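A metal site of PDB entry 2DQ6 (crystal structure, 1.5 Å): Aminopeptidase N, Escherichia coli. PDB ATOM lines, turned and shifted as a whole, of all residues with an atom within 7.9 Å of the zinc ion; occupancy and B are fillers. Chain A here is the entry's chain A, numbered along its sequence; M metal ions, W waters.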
ATOM      1  N   GLU A 121       1.768  21.975  37.164  1.00  0.00           N
ATOM      2  CA  GLU A 121       2.507  20.726  37.266  1.00  0.00           C
ATOM      3  C   GLU A 121       4.015  20.984  37.249  1.00  0.00           C
ATOM      4  O   GLU A 121       4.349  21.846  36.441  1.00  0.00           O
ATOM      5  CB  GLU A 121       2.136  19.798  36.110  1.00  0.00           C
ATOM      6  CG  GLU A 121       2.757  18.413  36.206  1.00  0.00           C
ATOM      7  CD  GLU A 121       2.479  17.559  34.978  1.00  0.00           C
ATOM      8  OE1 GLU A 121       2.790  16.351  35.013  1.00  0.00           O
ATOM      9  OE2 GLU A 121       1.955  18.110  33.986  1.00  0.00           O
ATOM     10  N   ALA A 262       2.039  21.930  26.276  1.00  0.00           N
ATOM     11  CA  ALA A 262       0.624  22.029  26.619  1.00  0.00           C
ATOM     12  C   ALA A 262       0.405  21.338  27.969  1.00  0.00           C
ATOM     13  O   ALA A 262       1.298  20.655  28.458  1.00  0.00           O
ATOM     14  CB  ALA A 262      -0.239  21.387  25.532  1.00  0.00           C
ATOM     15  N   MET A 263      -0.779  21.509  28.545  1.00  0.00           N
ATOM     16  CA  MET A 263      -1.079  20.936  29.849  1.00  0.00           C
ATOM     17  C   MET A 263      -2.515  20.449  29.926  1.00  0.00           C
ATOM     18  O   MET A 263      -3.455  21.188  29.583  1.00  0.00           O
ATOM     19  CB  MET A 263      -0.804  21.973  30.931  1.00  0.00           C
ATOM     20  CG  MET A 263      -0.996  21.473  32.350  1.00  0.00           C
ATOM     21  SD  MET A 263       0.114  20.103  32.759  1.00  0.00           S
ATOM     22  CE  MET A 263      -0.916  19.205  33.907  1.00  0.00           C
ATOM     23  N   GLU A 264      -2.684  19.221  30.410  1.00  0.00           N
ATOM     24  CA  GLU A 264      -3.990  18.569  30.495  1.00  0.00           C
ATOM     25  C   GLU A 264      -4.927  18.903  31.661  1.00  0.00           C
ATOM     26  O   GLU A 264      -5.701  18.051  32.078  1.00  0.00           O
ATOM     27  CB  GLU A 264      -3.784  17.049  30.455  1.00  0.00           C
ATOM     28  CG  GLU A 264      -3.175  16.435  31.739  1.00  0.00           C
ATOM     29  CD  GLU A 264      -1.649  16.410  31.781  1.00  0.00           C
ATOM     30  OE1 GLU A 264      -1.101  15.654  32.606  1.00  0.00           O
ATOM     31  OE2 GLU A 264      -0.990  17.144  31.004  1.00  0.00           O
ATOM     32  N   VAL A 294      -0.484  17.069  19.649  1.00  0.00           N
ATOM     33  CA  VAL A 294      -0.562  17.615  20.990  1.00  0.00           C
ATOM     34  C   VAL A 294      -1.999  17.829  21.470  1.00  0.00           C
ATOM     35  O   VAL A 294      -2.304  17.584  22.634  1.00  0.00           O
ATOM     36  CB  VAL A 294       0.281  18.908  21.096  1.00  0.00           C
ATOM     37  CG1 VAL A 294       0.179  19.506  22.488  1.00  0.00           C
ATOM     38  CG2 VAL A 294       1.750  18.581  20.787  1.00  0.00           C
ATOM     39  N   HIS A 297      -2.874  14.439  22.379  1.00  0.00           N
ATOM     40  CA  HIS A 297      -2.155  14.074  23.594  1.00  0.00           C
ATOM     41  C   HIS A 297      -2.823  14.572  24.868  1.00  0.00           C
ATOM     42  O   HIS A 297      -3.121  13.783  25.774  1.00  0.00           O
ATOM     43  CB  HIS A 297      -0.733  14.635  23.516  1.00  0.00           C
ATOM     44  CG  HIS A 297       0.136  14.239  24.672  1.00  0.00           C
ATOM     45  ND1 HIS A 297       1.011  13.165  24.618  1.00  0.00           N
ATOM     46  CD2 HIS A 297       0.264  14.755  25.912  1.00  0.00           C
ATOM     47  CE1 HIS A 297       1.627  13.049  25.778  1.00  0.00           C
ATOM     48  NE2 HIS A 297       1.192  14.004  26.580  1.00  0.00           N
ATOM     49  N   GLU A 298      -3.085  15.877  24.941  1.00  0.00           N
ATOM     50  CA  GLU A 298      -3.692  16.423  26.147  1.00  0.00           C
ATOM     51  C   GLU A 298      -5.101  15.858  26.351  1.00  0.00           C
ATOM     52  O   GLU A 298      -5.511  15.624  27.489  1.00  0.00           O
ATOM     53  CB  GLU A 298      -3.727  17.949  26.106  1.00  0.00           C
ATOM     54  CG  GLU A 298      -2.369  18.629  25.835  1.00  0.00           C
ATOM     55  CD  GLU A 298      -1.184  18.031  26.591  1.00  0.00           C
ATOM     56  OE1 GLU A 298      -1.370  17.492  27.699  1.00  0.00           O
ATOM     57  OE2 GLU A 298      -0.052  18.142  26.088  1.00  0.00           O
ATOM     58  N   PHE A 300      -6.139  12.868  25.441  1.00  0.00           N
ATOM     59  CA  PHE A 300      -5.989  11.488  25.890  1.00  0.00           C
ATOM     60  C   PHE A 300      -5.644  11.399  27.379  1.00  0.00           C
ATOM     61  O   PHE A 300      -5.950  10.398  28.032  1.00  0.00           O
ATOM     62  CB  PHE A 300      -4.942  10.785  25.014  1.00  0.00           C
ATOM     63  CG  PHE A 300      -5.292  10.784  23.552  1.00  0.00           C
ATOM     64  CD1 PHE A 300      -4.294  10.819  22.575  1.00  0.00           C
ATOM     65  CD2 PHE A 300      -6.631  10.792  23.149  1.00  0.00           C
ATOM     66  CE1 PHE A 300      -4.626  10.881  21.216  1.00  0.00           C
ATOM     67  CE2 PHE A 300      -6.975  10.859  21.795  1.00  0.00           C
ATOM     68  CZ  PHE A 300      -5.968  10.905  20.828  1.00  0.00           C
ATOM     69  N   HIS A 301      -5.014  12.441  27.902  1.00  0.00           N
ATOM     70  CA  HIS A 301      -4.682  12.482  29.324  1.00  0.00           C
ATOM     71  C   HIS A 301      -5.947  12.496  30.168  1.00  0.00           C
ATOM     72  O   HIS A 301      -5.890  12.185  31.362  1.00  0.00           O
ATOM     73  CB  HIS A 301      -3.891  13.752  29.671  1.00  0.00           C
ATOM     74  CG  HIS A 301      -2.415  13.574  29.669  1.00  0.00           C
ATOM     75  ND1 HIS A 301      -1.779  12.570  30.361  1.00  0.00           N
ATOM     76  CD2 HIS A 301      -1.429  14.314  29.100  1.00  0.00           C
ATOM     77  CE1 HIS A 301      -0.470  12.699  30.219  1.00  0.00           C
ATOM     78  NE2 HIS A 301      -0.239  13.750  29.462  1.00  0.00           N
ATOM     79  N   THR A 304      -5.891   8.776  30.767  1.00  0.00           N
ATOM     80  CA  THR A 304      -4.576   8.335  31.182  1.00  0.00           C
ATOM     81  C   THR A 304      -3.785   9.509  31.781  1.00  0.00           C
ATOM     82  O   THR A 304      -2.898  10.086  31.141  1.00  0.00           O
ATOM     83  CB  THR A 304      -3.823   7.655  30.016  1.00  0.00           C
ATOM     84  OG1 THR A 304      -3.798   8.517  28.866  1.00  0.00           O
ATOM     85  CG2 THR A 304      -4.535   6.365  29.626  1.00  0.00           C
ATOM     86  N   LEU A 316       5.651   9.364  36.919  1.00  0.00           N
ATOM     87  CA  LEU A 316       5.275  10.213  35.790  1.00  0.00           C
ATOM     88  C   LEU A 316       5.024   9.467  34.476  1.00  0.00           C
ATOM     89  O   LEU A 316       4.067   9.769  33.765  1.00  0.00           O
ATOM     90  CB  LEU A 316       6.330  11.296  35.565  1.00  0.00           C
ATOM     91  CG  LEU A 316       6.061  12.301  34.439  1.00  0.00           C
ATOM     92  CD1 LEU A 316       4.735  13.031  34.697  1.00  0.00           C
ATOM     93  CD2 LEU A 316       7.201  13.298  34.372  1.00  0.00           C
ATOM     94  N   LYS A 319       1.580   8.091  33.181  1.00  0.00           N
ATOM     95  CA  LYS A 319       0.682   8.877  32.347  1.00  0.00           C
ATOM     96  C   LYS A 319       1.360   9.378  31.077  1.00  0.00           C
ATOM     97  O   LYS A 319       0.745   9.383  30.014  1.00  0.00           O
ATOM     98  CB  LYS A 319       0.056  10.044  33.129  1.00  0.00           C
ATOM     99  CG  LYS A 319       0.975  11.208  33.539  1.00  0.00           C
ATOM    100  CD  LYS A 319       0.129  12.265  34.281  1.00  0.00           C
ATOM    101  CE  LYS A 319       0.938  13.467  34.782  1.00  0.00           C
ATOM    102  NZ  LYS A 319       1.274  14.432  33.701  1.00  0.00           N
ATOM    103  N   GLU A 320       2.631   9.770  31.150  1.00  0.00           N
ATOM    104  CA  GLU A 320       3.293  10.296  29.955  1.00  0.00           C
ATOM    105  C   GLU A 320       3.664   9.249  28.910  1.00  0.00           C
ATOM    106  O   GLU A 320       3.451   9.461  27.721  1.00  0.00           O
ATOM    107  CB  GLU A 320       4.519  11.129  30.343  1.00  0.00           C
ATOM    108  CG  GLU A 320       4.173  12.334  31.215  1.00  0.00           C
ATOM    109  CD  GLU A 320       3.146  13.252  30.571  1.00  0.00           C
ATOM    110  OE1 GLU A 320       2.559  14.081  31.296  1.00  0.00           O
ATOM    111  OE2 GLU A 320       2.942  13.175  29.345  1.00  0.00           O
ATOM    112  N   GLY A 321       4.213   8.118  29.339  1.00  0.00           N
ATOM    113  CA  GLY A 321       4.566   7.081  28.378  1.00  0.00           C
ATOM    114  C   GLY A 321       3.319   6.552  27.699  1.00  0.00           C
ATOM    115  O   GLY A 321       3.272   6.391  26.476  1.00  0.00           O
ATOM    116  N   LEU A 322       2.286   6.282  28.493  1.00  0.00           N
ATOM    117  CA  LEU A 322       1.025   5.766  27.961  1.00  0.00           C
ATOM    118  C   LEU A 322       0.297   6.785  27.078  1.00  0.00           C
ATOM    119  O   LEU A 322      -0.290   6.412  26.063  1.00  0.00           O
ATOM    120  CB  LEU A 322       0.126   5.326  29.117  1.00  0.00           C
ATOM    121  CG  LEU A 322      -1.250   4.731  28.784  1.00  0.00           C
ATOM    122  CD1 LEU A 322      -1.113   3.550  27.820  1.00  0.00           C
ATOM    123  CD2 LEU A 322      -1.897   4.277  30.085  1.00  0.00           C
ATOM    124  N   THR A 323       0.349   8.059  27.454  1.00  0.00           N
ATOM    125  CA  THR A 323      -0.332   9.078  26.662  1.00  0.00           C
ATOM    126  C   THR A 323       0.442   9.376  25.372  1.00  0.00           C
ATOM    127  O   THR A 323      -0.165   9.686  24.354  1.00  0.00           O
ATOM    128  CB  THR A 323      -0.568  10.342  27.495  1.00  0.00           C
ATOM    129  OG1 THR A 323      -1.387  10.002  28.619  1.00  0.00           O
ATOM    130  CG2 THR A 323      -1.292  11.409  26.673  1.00  0.00           C
ATOM    131  N   VAL A 324       1.769   9.269  25.416  1.00  0.00           N
ATOM    132  CA  VAL A 324       2.548   9.477  24.195  1.00  0.00           C
ATOM    133  C   VAL A 324       2.231   8.304  23.264  1.00  0.00           C
ATOM    134  O   VAL A 324       2.050   8.490  22.058  1.00  0.00           O
ATOM    135  CB  VAL A 324       4.064   9.528  24.470  1.00  0.00           C
ATOM    136  CG1 VAL A 324       4.841   9.392  23.162  1.00  0.00           C
ATOM    137  CG2 VAL A 324       4.419  10.852  25.135  1.00  0.00           C
ATOM    138  N   ASP A 327      -0.960   9.123  21.672  1.00  0.00           N
ATOM    139  CA  ASP A 327      -0.934  10.132  20.624  1.00  0.00           C
ATOM    140  C   ASP A 327      -0.251   9.613  19.363  1.00  0.00           C
ATOM    141  O   ASP A 327      -0.606  10.020  18.262  1.00  0.00           O
ATOM    142  CB  ASP A 327      -0.348  11.488  21.137  1.00  0.00           C
ATOM    143  CG  ASP A 327       1.187  11.551  21.160  1.00  0.00           C
ATOM    144  OD1 ASP A 327       1.734  12.031  22.178  1.00  0.00           O
ATOM    145  OD2 ASP A 327       1.848  11.195  20.164  1.00  0.00           O
ATOM    146  N   TYR A 376      10.759  15.723  32.857  1.00  0.00           N
ATOM    147  CA  TYR A 376       9.749  15.676  31.807  1.00  0.00           C
ATOM    148  C   TYR A 376      10.654  15.517  30.589  1.00  0.00           C
ATOM    149  O   TYR A 376      10.857  16.436  29.785  1.00  0.00           O
ATOM    150  CB  TYR A 376       8.950  16.974  31.790  1.00  0.00           C
ATOM    151  CG  TYR A 376       7.969  16.992  32.933  1.00  0.00           C
ATOM    152  CD1 TYR A 376       8.412  17.101  34.252  1.00  0.00           C
ATOM    153  CD2 TYR A 376       6.614  16.747  32.725  1.00  0.00           C
ATOM    154  CE1 TYR A 376       7.538  16.960  35.327  1.00  0.00           C
ATOM    155  CE2 TYR A 376       5.728  16.596  33.780  1.00  0.00           C
ATOM    156  CZ  TYR A 376       6.201  16.702  35.077  1.00  0.00           C
ATOM    157  OH  TYR A 376       5.343  16.495  36.133  1.00  0.00           O
ATOM    158  N   TYR A 381       8.953  10.276  28.537  1.00  0.00           N
ATOM    159  CA  TYR A 381       7.928  10.378  27.499  1.00  0.00           C
ATOM    160  C   TYR A 381       8.097   9.384  26.353  1.00  0.00           C
ATOM    161  O   TYR A 381       7.302   8.455  26.202  1.00  0.00           O
ATOM    162  CB  TYR A 381       7.924  11.793  26.886  1.00  0.00           C
ATOM    163  CG  TYR A 381       7.186  12.844  27.674  1.00  0.00           C
ATOM    164  CD1 TYR A 381       7.582  13.209  28.951  1.00  0.00           C
ATOM    165  CD2 TYR A 381       6.101  13.522  27.102  1.00  0.00           C
ATOM    166  CE1 TYR A 381       6.917  14.228  29.654  1.00  0.00           C
ATOM    167  CE2 TYR A 381       5.436  14.534  27.793  1.00  0.00           C
ATOM    168  CZ  TYR A 381       5.849  14.886  29.061  1.00  0.00           C
ATOM    169  OH  TYR A 381       5.205  15.891  29.732  1.00  0.00           O
HETATM  170 ZN    ZN M   1       1.528  14.393  28.584  1.00  0.00          ZN
HETATM  171  O   HOH W   1       1.286  16.613  28.587  1.00  0.00           O
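A ring nitrogen (ND1) of His 297 lies within hydrogen-bond range of the side-chain carboxylate (OD1) of Asp 327, 2.8 Å away.
The side-chain amino group (NZ) of Lys 319 lies within salt-bridge range of the side-chain carboxylate (OE1) of Glu 320 (2.7 Å).
ND1 of His 301 is in hydrogen-bond range of OG1 of Thr 323 (3.1 Å).
A ring nitrogen (ND1) of His 301 lies within hydrogen-bond range of the backbone carbonyl oxygen (O) of Thr 304 (2.8 Å).
CE2 of Tyr 381 touches the zinc ion (3.99 Å).
The nearest printed residue that does not touch the zinc ion is Glu 298 (4.3 Å).
The zinc ion is bound by the side-chain carboxylate of Glu 320 (2.0 Å), a ring nitrogen (NE2) of His 297 (2.1 Å), a ring nitrogen (NE2) of His 301 (2.1 Å) and water W1 (2.2 Å).
The zinc ion has four donor atoms within binding distance.
Water W1 lies within hydrogen-bond range of the side-chain carboxylate (OE1) of Glu 298 (2.9 Å) and the side-chain carboxylate (OE2) of Glu 264 (3.4 Å).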
